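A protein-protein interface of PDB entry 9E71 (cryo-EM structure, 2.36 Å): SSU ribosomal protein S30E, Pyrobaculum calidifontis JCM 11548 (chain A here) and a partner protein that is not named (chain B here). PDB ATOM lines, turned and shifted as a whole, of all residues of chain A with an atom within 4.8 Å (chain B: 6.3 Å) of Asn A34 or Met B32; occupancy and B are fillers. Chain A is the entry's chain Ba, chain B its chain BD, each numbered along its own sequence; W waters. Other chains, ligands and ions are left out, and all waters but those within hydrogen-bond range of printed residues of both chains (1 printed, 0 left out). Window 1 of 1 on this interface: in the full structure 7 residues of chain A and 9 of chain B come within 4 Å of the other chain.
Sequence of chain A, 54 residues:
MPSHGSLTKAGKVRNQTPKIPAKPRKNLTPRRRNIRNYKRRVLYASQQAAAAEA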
ATOM      1  N   PRO A  30     -13.962  -4.832 -16.320  1.00  0.00           N
ATOM      2  CA  PRO A  30     -14.982  -3.898 -15.798  1.00  0.00           C
ATOM      3  C   PRO A  30     -16.251  -4.558 -15.280  1.00  0.00           C
ATOM      4  O   PRO A  30     -16.781  -4.149 -14.238  1.00  0.00           O
ATOM      5  CB  PRO A  30     -15.265  -3.002 -17.010  1.00  0.00           C
ATOM      6  CG  PRO A  30     -14.050  -3.079 -17.843  1.00  0.00           C
ATOM      7  CD  PRO A  30     -13.482  -4.443 -17.656  1.00  0.00           C
ATOM      8  N   ARG A  31     -16.730  -5.594 -15.965  1.00  0.00           N
ATOM      9  CA  ARG A  31     -17.942  -6.280 -15.532  1.00  0.00           C
ATOM     10  C   ARG A  31     -17.730  -6.979 -14.196  1.00  0.00           C
ATOM     11  O   ARG A  31     -18.558  -6.871 -13.283  1.00  0.00           O
ATOM     12  CB  ARG A  31     -18.372  -7.277 -16.605  1.00  0.00           C
ATOM     13  CG  ARG A  31     -19.856  -7.307 -16.873  1.00  0.00           C
ATOM     14  CD  ARG A  31     -20.216  -8.522 -17.702  1.00  0.00           C
ATOM     15  NE  ARG A  31     -20.058  -9.754 -16.939  1.00  0.00           N
ATOM     16  CZ  ARG A  31     -19.237 -10.739 -17.272  1.00  0.00           C
ATOM     17  NH1 ARG A  31     -18.491 -10.678 -18.361  1.00  0.00           N
ATOM     18  NH2 ARG A  31     -19.160 -11.811 -16.490  1.00  0.00           N
ATOM     19  N   ARG A  32     -16.606  -7.682 -14.052  1.00  0.00           N
ATOM     20  CA  ARG A  32     -16.316  -8.362 -12.798  1.00  0.00           C
ATOM     21  C   ARG A  32     -16.052  -7.375 -11.669  1.00  0.00           C
ATOM     22  O   ARG A  32     -16.414  -7.643 -10.520  1.00  0.00           O
ATOM     23  CB  ARG A  32     -15.129  -9.301 -12.976  1.00  0.00           C
ATOM     24  CG  ARG A  32     -15.328 -10.318 -14.075  1.00  0.00           C
ATOM     25  CD  ARG A  32     -15.628 -11.682 -13.498  1.00  0.00           C
ATOM     26  NE  ARG A  32     -14.948 -11.888 -12.225  1.00  0.00           N
ATOM     27  CZ  ARG A  32     -14.013 -12.804 -12.017  1.00  0.00           C
ATOM     28  NH1 ARG A  32     -13.619 -13.621 -12.978  1.00  0.00           N
ATOM     29  NH2 ARG A  32     -13.458 -12.900 -10.813  1.00  0.00           N
ATOM     30  N   ARG A  33     -15.426  -6.238 -11.969  1.00  0.00           N
ATOM     31  CA  ARG A  33     -15.209  -5.229 -10.939  1.00  0.00           C
ATOM     32  C   ARG A  33     -16.525  -4.645 -10.449  1.00  0.00           C
ATOM     33  O   ARG A  33     -16.713  -4.443  -9.244  1.00  0.00           O
ATOM     34  CB  ARG A  33     -14.312  -4.120 -11.470  1.00  0.00           C
ATOM     35  CG  ARG A  33     -14.214  -2.912 -10.568  1.00  0.00           C
ATOM     36  CD  ARG A  33     -14.412  -1.627 -11.338  1.00  0.00           C
ATOM     37  NE  ARG A  33     -14.412  -0.469 -10.455  1.00  0.00           N
ATOM     38  CZ  ARG A  33     -15.043   0.669 -10.705  1.00  0.00           C
ATOM     39  NH1 ARG A  33     -15.733   0.844 -11.818  1.00  0.00           N
ATOM     40  NH2 ARG A  33     -14.976   1.656  -9.819  1.00  0.00           N
ATOM     41  N   ASN A  34     -17.442  -4.353 -11.371  1.00  0.00           N
ATOM     42  CA  ASN A  34     -18.743  -3.844 -10.959  1.00  0.00           C
ATOM     43  C   ASN A  34     -19.522  -4.900 -10.185  1.00  0.00           C
ATOM     44  O   ASN A  34     -20.241  -4.572  -9.232  1.00  0.00           O
ATOM     45  CB  ASN A  34     -19.520  -3.360 -12.177  1.00  0.00           C
ATOM     46  CG  ASN A  34     -18.984  -2.053 -12.720  1.00  0.00           C
ATOM     47  OD1 ASN A  34     -18.432  -2.000 -13.817  1.00  0.00           O
ATOM     48  ND2 ASN A  34     -19.134  -0.990 -11.946  1.00  0.00           N
ATOM     49  N   ILE A  35     -19.364  -6.174 -10.559  1.00  0.00           N
ATOM     50  CA  ILE A  35     -19.985  -7.265  -9.808  1.00  0.00           C
ATOM     51  C   ILE A  35     -19.446  -7.310  -8.384  1.00  0.00           C
ATOM     52  O   ILE A  35     -20.205  -7.453  -7.419  1.00  0.00           O
ATOM     53  CB  ILE A  35     -19.757  -8.606 -10.524  1.00  0.00           C
ATOM     54  CG1 ILE A  35     -20.858  -8.871 -11.541  1.00  0.00           C
ATOM     55  CG2 ILE A  35     -19.681  -9.740  -9.517  1.00  0.00           C
ATOM     56  CD1 ILE A  35     -20.515  -9.968 -12.501  1.00  0.00           C
ATOM     57  N   ARG A  36     -18.125  -7.194  -8.239  1.00  0.00           N
ATOM     58  CA  ARG A  36     -17.501  -7.240  -6.921  1.00  0.00           C
ATOM     59  C   ARG A  36     -17.948  -6.070  -6.057  1.00  0.00           C
ATOM     60  O   ARG A  36     -18.236  -6.236  -4.866  1.00  0.00           O
ATOM     61  CB  ARG A  36     -15.980  -7.242  -7.064  1.00  0.00           C
ATOM     62  CG  ARG A  36     -15.247  -7.519  -5.770  1.00  0.00           C
ATOM     63  CD  ARG A  36     -13.919  -6.795  -5.710  1.00  0.00           C
ATOM     64  NE  ARG A  36     -13.911  -5.577  -6.504  1.00  0.00           N
ATOM     65  CZ  ARG A  36     -12.823  -5.048  -7.044  1.00  0.00           C
ATOM     66  NH1 ARG A  36     -11.637  -5.614  -6.903  1.00  0.00           N
ATOM     67  NH2 ARG A  36     -12.928  -3.923  -7.742  1.00  0.00           N
ATOM     68  N   ASN A  37     -18.009  -4.874  -6.646  1.00  0.00           N
ATOM     69  CA  ASN A  37     -18.413  -3.697  -5.884  1.00  0.00           C
ATOM     70  C   ASN A  37     -19.872  -3.781  -5.460  1.00  0.00           C
ATOM     71  O   ASN A  37     -20.218  -3.412  -4.333  1.00  0.00           O
ATOM     72  CB  ASN A  37     -18.160  -2.436  -6.700  1.00  0.00           C
ATOM     73  CG  ASN A  37     -16.712  -2.284  -7.087  1.00  0.00           C
ATOM     74  OD1 ASN A  37     -15.876  -3.112  -6.734  1.00  0.00           O
ATOM     75  ND2 ASN A  37     -16.403  -1.219  -7.816  1.00  0.00           N
ATOM     76  N   TYR A  38     -20.746  -4.265  -6.349  1.00  0.00           N
ATOM     77  CA  TYR A  38     -22.138  -4.478  -5.969  1.00  0.00           C
ATOM     78  C   TYR A  38     -22.261  -5.531  -4.877  1.00  0.00           C
ATOM     79  O   TYR A  38     -23.089  -5.401  -3.968  1.00  0.00           O
ATOM     80  CB  TYR A  38     -22.959  -4.894  -7.183  1.00  0.00           C
ATOM     81  CG  TYR A  38     -24.440  -4.926  -6.919  1.00  0.00           C
ATOM     82  CD1 TYR A  38     -25.131  -3.765  -6.633  1.00  0.00           C
ATOM     83  CD2 TYR A  38     -25.151  -6.113  -6.975  1.00  0.00           C
ATOM     84  CE1 TYR A  38     -26.485  -3.780  -6.398  1.00  0.00           C
ATOM     85  CE2 TYR A  38     -26.508  -6.140  -6.741  1.00  0.00           C
ATOM     86  CZ  TYR A  38     -27.169  -4.969  -6.454  1.00  0.00           C
ATOM     87  OH  TYR A  38     -28.523  -4.982  -6.219  1.00  0.00           O
ATOM     88  N   GLU B  27     -25.621   5.387  -5.867  1.00  0.00           N
ATOM     89  CA  GLU B  27     -26.770   5.124  -6.733  1.00  0.00           C
ATOM     90  C   GLU B  27     -26.358   4.506  -8.066  1.00  0.00           C
ATOM     91  O   GLU B  27     -27.036   3.600  -8.575  1.00  0.00           O
ATOM     92  CB  GLU B  27     -27.574   6.403  -6.946  1.00  0.00           C
ATOM     93  CG  GLU B  27     -28.647   6.688  -5.894  1.00  0.00           C
ATOM     94  CD  GLU B  27     -28.110   7.064  -4.525  1.00  0.00           C
ATOM     95  OE1 GLU B  27     -28.833   7.751  -3.774  1.00  0.00           O
ATOM     96  OE2 GLU B  27     -27.014   6.604  -4.154  1.00  0.00           O
ATOM     97  N   GLU B  28     -25.249   4.972  -8.647  1.00  0.00           N
ATOM     98  CA  GLU B  28     -24.788   4.383  -9.899  1.00  0.00           C
ATOM     99  C   GLU B  28     -24.354   2.938  -9.706  1.00  0.00           C
ATOM    100  O   GLU B  28     -24.623   2.085 -10.557  1.00  0.00           O
ATOM    101  CB  GLU B  28     -23.653   5.221 -10.481  1.00  0.00           C
ATOM    102  CG  GLU B  28     -24.114   6.550 -11.041  1.00  0.00           C
ATOM    103  CD  GLU B  28     -23.145   7.130 -12.045  1.00  0.00           C
ATOM    104  OE1 GLU B  28     -22.000   6.643 -12.122  1.00  0.00           O
ATOM    105  OE2 GLU B  28     -23.534   8.067 -12.768  1.00  0.00           O
ATOM    106  N   LEU B  29     -23.695   2.642  -8.585  1.00  0.00           N
ATOM    107  CA  LEU B  29     -23.295   1.273  -8.290  1.00  0.00           C
ATOM    108  C   LEU B  29     -24.506   0.374  -8.100  1.00  0.00           C
ATOM    109  O   LEU B  29     -24.503  -0.787  -8.531  1.00  0.00           O
ATOM    110  CB  LEU B  29     -22.410   1.260  -7.048  1.00  0.00           C
ATOM    111  CG  LEU B  29     -22.088  -0.087  -6.428  1.00  0.00           C
ATOM    112  CD1 LEU B  29     -21.536  -1.027  -7.476  1.00  0.00           C
ATOM    113  CD2 LEU B  29     -21.089   0.114  -5.312  1.00  0.00           C
ATOM    114  N   GLN B  30     -25.555   0.901  -7.462  1.00  0.00           N
ATOM    115  CA  GLN B  30     -26.786   0.142  -7.270  1.00  0.00           C
ATOM    116  C   GLN B  30     -27.417  -0.199  -8.611  1.00  0.00           C
ATOM    117  O   GLN B  30     -27.809  -1.346  -8.849  1.00  0.00           O
ATOM    118  CB  GLN B  30     -27.716   0.946  -6.339  1.00  0.00           C
ATOM    119  CG  GLN B  30     -29.169   0.481  -5.944  1.00  0.00           C
ATOM    120  CD  GLN B  30     -30.330   0.569  -6.966  1.00  0.00           C
ATOM    121  OE1 GLN B  30     -30.170   0.585  -8.176  1.00  0.00           O
ATOM    122  NE2 GLN B  30     -31.539   0.614  -6.423  1.00  0.00           N
ATOM    123  N   LEU B  31     -27.517   0.790  -9.504  1.00  0.00           N
ATOM    124  CA  LEU B  31     -28.103   0.549 -10.822  1.00  0.00           C
ATOM    125  C   LEU B  31     -27.278  -0.450 -11.625  1.00  0.00           C
ATOM    126  O   LEU B  31     -27.825  -1.360 -12.266  1.00  0.00           O
ATOM    127  CB  LEU B  31     -28.230   1.867 -11.586  1.00  0.00           C
ATOM    128  CG  LEU B  31     -29.499   2.667 -11.315  1.00  0.00           C
ATOM    129  CD1 LEU B  31     -29.410   4.049 -11.929  1.00  0.00           C
ATOM    130  CD2 LEU B  31     -30.711   1.913 -11.838  1.00  0.00           C
ATOM    131  N   MET B  32     -25.951  -0.290 -11.588  1.00  0.00           N
ATOM    132  CA  MET B  32     -25.051  -1.175 -12.318  1.00  0.00           C
ATOM    133  C   MET B  32     -25.173  -2.610 -11.837  1.00  0.00           C
ATOM    134  O   MET B  32     -25.226  -3.543 -12.643  1.00  0.00           O
ATOM    135  CB  MET B  32     -23.616  -0.676 -12.167  1.00  0.00           C
ATOM    136  CG  MET B  32     -22.627  -1.239 -13.163  1.00  0.00           C
ATOM    137  SD  MET B  32     -22.464  -0.114 -14.546  1.00  0.00           S
ATOM    138  CE  MET B  32     -22.498   1.428 -13.661  1.00  0.00           C
ATOM    139  N   GLY B  33     -25.236  -2.807 -10.522  1.00  0.00           N
ATOM    140  CA  GLY B  33     -25.359  -4.158 -10.010  1.00  0.00           C
ATOM    141  C   GLY B  33     -26.732  -4.756 -10.236  1.00  0.00           C
ATOM    142  O   GLY B  33     -26.864  -5.971 -10.414  1.00  0.00           O
ATOM    143  N   GLU B  34     -27.775  -3.923 -10.212  1.00  0.00           N
ATOM    144  CA  GLU B  34     -29.121  -4.424 -10.466  1.00  0.00           C
ATOM    145  C   GLU B  34     -29.255  -4.933 -11.891  1.00  0.00           C
ATOM    146  O   GLU B  34     -29.778  -6.028 -12.124  1.00  0.00           O
ATOM    147  CB  GLU B  34     -30.154  -3.332 -10.197  1.00  0.00           C
ATOM    148  CG  GLU B  34     -30.339  -2.978  -8.737  1.00  0.00           C
ATOM    149  CD  GLU B  34     -31.600  -2.179  -8.495  1.00  0.00           C
ATOM    150  OE1 GLU B  34     -32.084  -1.532  -9.446  1.00  0.00           O
ATOM    151  OE2 GLU B  34     -32.105  -2.193  -7.355  1.00  0.00           O
ATOM    152  N   TYR B  35     -28.780  -4.158 -12.864  1.00  0.00           N
ATOM    153  CA  TYR B  35     -29.008  -4.510 -14.258  1.00  0.00           C
ATOM    154  C   TYR B  35     -27.827  -5.207 -14.920  1.00  0.00           C
ATOM    155  O   TYR B  35     -27.913  -5.524 -16.109  1.00  0.00           O
ATOM    156  CB  TYR B  35     -29.393  -3.266 -15.049  1.00  0.00           C
ATOM    157  CG  TYR B  35     -30.710  -2.682 -14.604  1.00  0.00           C
ATOM    158  CD1 TYR B  35     -31.906  -3.304 -14.920  1.00  0.00           C
ATOM    159  CD2 TYR B  35     -30.755  -1.523 -13.848  1.00  0.00           C
ATOM    160  CE1 TYR B  35     -33.109  -2.776 -14.512  1.00  0.00           C
ATOM    161  CE2 TYR B  35     -31.954  -0.991 -13.434  1.00  0.00           C
ATOM    162  CZ  TYR B  35     -33.127  -1.621 -13.768  1.00  0.00           C
ATOM    163  OH  TYR B  35     -34.323  -1.090 -13.357  1.00  0.00           O
ATOM    164  N   GLY B  36     -26.748  -5.472 -14.192  1.00  0.00           N
ATOM    165  CA  GLY B  36     -25.627  -6.208 -14.760  1.00  0.00           C
ATOM    166  C   GLY B  36     -24.920  -5.510 -15.903  1.00  0.00           C
ATOM    167  O   GLY B  36     -24.571  -6.155 -16.900  1.00  0.00           O
ATOM    168  N   LEU B  37     -24.699  -4.207 -15.784  1.00  0.00           N
ATOM    169  CA  LEU B  37     -24.071  -3.449 -16.851  1.00  0.00           C
ATOM    170  C   LEU B  37     -22.562  -3.676 -16.862  1.00  0.00           C
ATOM    171  O   LEU B  37     -21.940  -3.943 -15.831  1.00  0.00           O
ATOM    172  CB  LEU B  37     -24.379  -1.966 -16.692  1.00  0.00           C
ATOM    173  CG  LEU B  37     -25.856  -1.650 -16.481  1.00  0.00           C
ATOM    174  CD1 LEU B  37     -26.021  -0.261 -15.906  1.00  0.00           C
ATOM    175  CD2 LEU B  37     -26.611  -1.788 -17.784  1.00  0.00           C
ATOM    176  N   ARG B  38     -21.972  -3.560 -18.053  1.00  0.00           N
ATOM    177  CA  ARG B  38     -20.544  -3.822 -18.205  1.00  0.00           C
ATOM    178  C   ARG B  38     -19.697  -2.745 -17.545  1.00  0.00           C
ATOM    179  O   ARG B  38     -18.759  -3.051 -16.803  1.00  0.00           O
ATOM    180  CB  ARG B  38     -20.180  -3.934 -19.682  1.00  0.00           C
ATOM    181  CG  ARG B  38     -18.709  -4.188 -19.909  1.00  0.00           C
ATOM    182  CD  ARG B  38     -18.395  -4.337 -21.379  1.00  0.00           C
ATOM    183  NE  ARG B  38     -17.128  -3.710 -21.726  1.00  0.00           N
ATOM    184  CZ  ARG B  38     -16.101  -4.353 -22.262  1.00  0.00           C
ATOM    185  NH1 ARG B  38     -16.155  -5.649 -22.516  1.00  0.00           N
ATOM    186  NH2 ARG B  38     -14.990  -3.680 -22.544  1.00  0.00           N
ATOM    187  N   ASN B  39     -20.001  -1.479 -17.815  1.00  0.00           N
ATOM    188  CA  ASN B  39     -19.240  -0.377 -17.251  1.00  0.00           C
ATOM    189  C   ASN B  39     -20.158   0.822 -17.087  1.00  0.00           C
ATOM    190  O   ASN B  39     -21.345   0.774 -17.410  1.00  0.00           O
ATOM    191  CB  ASN B  39     -18.035  -0.007 -18.121  1.00  0.00           C
ATOM    192  CG  ASN B  39     -18.318  -0.140 -19.596  1.00  0.00           C
ATOM    193  OD1 ASN B  39     -19.001   0.692 -20.184  1.00  0.00           O
ATOM    194  ND2 ASN B  39     -17.770  -1.173 -20.209  1.00  0.00           N
ATOM    195  N   LYS B  40     -19.579   1.914 -16.585  1.00  0.00           N
ATOM    196  CA  LYS B  40     -20.334   3.140 -16.377  1.00  0.00           C
ATOM    197  C   LYS B  40     -20.788   3.775 -17.683  1.00  0.00           C
ATOM    198  O   LYS B  40     -21.743   4.558 -17.678  1.00  0.00           O
ATOM    199  CB  LYS B  40     -19.491   4.133 -15.580  1.00  0.00           C
ATOM    200  CG  LYS B  40     -19.064   3.637 -14.218  1.00  0.00           C
ATOM    201  CD  LYS B  40     -20.215   3.728 -13.241  1.00  0.00           C
ATOM    202  CE  LYS B  40     -19.789   4.263 -11.898  1.00  0.00           C
ATOM    203  NZ  LYS B  40     -20.766   3.966 -10.825  1.00  0.00           N
ATOM    204  N   LYS B  41     -20.123   3.459 -18.795  1.00  0.00           N
ATOM    205  CA  LYS B  41     -20.509   4.013 -20.087  1.00  0.00           C
ATOM    206  C   LYS B  41     -21.915   3.581 -20.482  1.00  0.00           C
ATOM    207  O   LYS B  41     -22.668   4.365 -21.064  1.00  0.00           O
ATOM    208  CB  LYS B  41     -19.504   3.583 -21.151  1.00  0.00           C
ATOM    209  CG  LYS B  41     -18.811   4.720 -21.853  1.00  0.00           C
ATOM    210  CD  LYS B  41     -17.861   4.190 -22.901  1.00  0.00           C
ATOM    211  CE  LYS B  41     -16.749   3.386 -22.260  1.00  0.00           C
ATOM    212  NZ  LYS B  41     -15.816   2.835 -23.274  1.00  0.00           N
ATOM    213  N   GLU B  42     -22.285   2.335 -20.178  1.00  0.00           N
ATOM    214  CA  GLU B  42     -23.631   1.862 -20.491  1.00  0.00           C
ATOM    215  C   GLU B  42     -24.687   2.623 -19.695  1.00  0.00           C
ATOM    216  O   GLU B  42     -25.721   3.034 -20.243  1.00  0.00           O
ATOM    217  CB  GLU B  42     -23.729   0.363 -20.218  1.00  0.00           C
ATOM    218  CG  GLU B  42     -22.947  -0.490 -21.200  1.00  0.00           C
ATOM    219  CD  GLU B  42     -22.938  -1.964 -20.829  1.00  0.00           C
ATOM    220  OE1 GLU B  42     -23.415  -2.311 -19.731  1.00  0.00           O
ATOM    221  OE2 GLU B  42     -22.454  -2.778 -21.642  1.00  0.00           O
ATOM    222  N   LEU B  43     -24.436   2.827 -18.400  1.00  0.00           N
ATOM    223  CA  LEU B  43     -25.364   3.582 -17.568  1.00  0.00           C
ATOM    224  C   LEU B  43     -25.477   5.022 -18.041  1.00  0.00           C
ATOM    225  O   LEU B  43     -26.573   5.597 -18.068  1.00  0.00           O
ATOM    226  CB  LEU B  43     -24.916   3.533 -16.109  1.00  0.00           C
ATOM    227  CG  LEU B  43     -25.775   4.330 -15.129  1.00  0.00           C
ATOM    228  CD1 LEU B  43     -27.202   3.829 -15.155  1.00  0.00           C
ATOM    229  CD2 LEU B  43     -25.201   4.254 -13.733  1.00  0.00           C
ATOM    230  N   HIS B 122     -26.590 -11.695 -15.274  1.00  0.00           N
ATOM    231  CA  HIS B 122     -25.325 -11.970 -15.939  1.00  0.00           C
ATOM    232  C   HIS B 122     -25.428 -13.196 -16.834  1.00  0.00           C
ATOM    233  O   HIS B 122     -24.806 -13.241 -17.901  1.00  0.00           O
ATOM    234  CB  HIS B 122     -24.223 -12.126 -14.898  1.00  0.00           C
ATOM    235  CG  HIS B 122     -23.991 -10.884 -14.099  1.00  0.00           C
ATOM    236  ND1 HIS B 122     -23.505  -9.723 -14.659  1.00  0.00           N
ATOM    237  CD2 HIS B 122     -24.203 -10.611 -12.790  1.00  0.00           C
ATOM    238  CE1 HIS B 122     -23.420  -8.789 -13.728  1.00  0.00           C
ATOM    239  NE2 HIS B 122     -23.833  -9.305 -12.584  1.00  0.00           N
HETATM  240  O   HOH W   1     -20.925  -5.811 -14.307  1.00  0.00           O
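The backbone carbonyl oxygen of Arg B38 lies close to the side-chain amide oxygen of Asn A34 (3.2 Å). O of Arg B38 is in hydrogen-bond range of N of Arg A31. O of Arg B38 sits close to O of Pro A30 (3.4 Å).
The side-chain amide oxygen (OD1) of Asn B39 sits close to the backbone NH (N) of Lys B41 (3.3 Å). The backbone NH of Arg B38 is in hydrogen-bond range of the side-chain carboxylate of Glu B42, 2.5 Å away. The backbone carbonyl oxygen (O) of Arg A33 sits close to the side-chain amide oxygen (OD1) of Asn A37 (3.0 Å). The guanidinium group of Arg A36 sits at hydrogen-bond distance from the side-chain amide oxygen of Asn A37. NE2 of Gln B30 sits at hydrogen-bond distance from OE2 of Glu B34 (3.0 Å). NE of Arg B38 sits close to ND2 of Asn B39.
Among the printed residues, pairs that only touch across the chains: Ile A35 with His B122 (3.2 Å), Tyr A38 with Gly B33 (3.3 Å), Tyr A38 with Leu B29 (3.5 Å), Tyr A38 with Glu B34 (3.7 Å), Tyr A38 with Gln B30 (3.7 Å), Asn A34 with Met B32 (3.7 Å), Asn A37 with Leu B29 (3.7 Å) and Asn A34 with Asn B39 (3.9 Å).
Printed residues of chain B within 4 Å of Arg A31: Arg B38 (3.4 Å). Printed residues of chain B within 4 Å of Asn A37: Leu B29. Of the printed residues of chain A, Gln B30 touches Tyr A38 (3.7 Å). The nearest printed residue of chain A that does not touch Met B32 is Tyr A38 (5.3 Å). The nearest printed residue of chain A that does not touch Arg B38 is Arg A32 (5.8 Å).
Of the 18 printed residues of chain B, 8 touch a printed residue of chain A. Printed residues of chain B that touch a printed residue of chain A: Leu B29, Gln B30, Met B32, Gly B33, Glu B34, Arg B38, Asn B39 and His B122. Hydrophobic or aromatic side chains of chain B that line the printed part of chain A: Leu B29, Met B32 and His B122. Among the printed residues, 11 pairs touch across the chains. Among the printed residues, no Asp or Glu carboxylate lies within 4 Å of a Lys or Arg side-chain nitrogen of the other chain.
Water W1 bridges the backbone carbonyl oxygen of Leu B37 (2.6 Å) and the backbone carbonyl oxygen of Arg A31 (2.8 Å).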
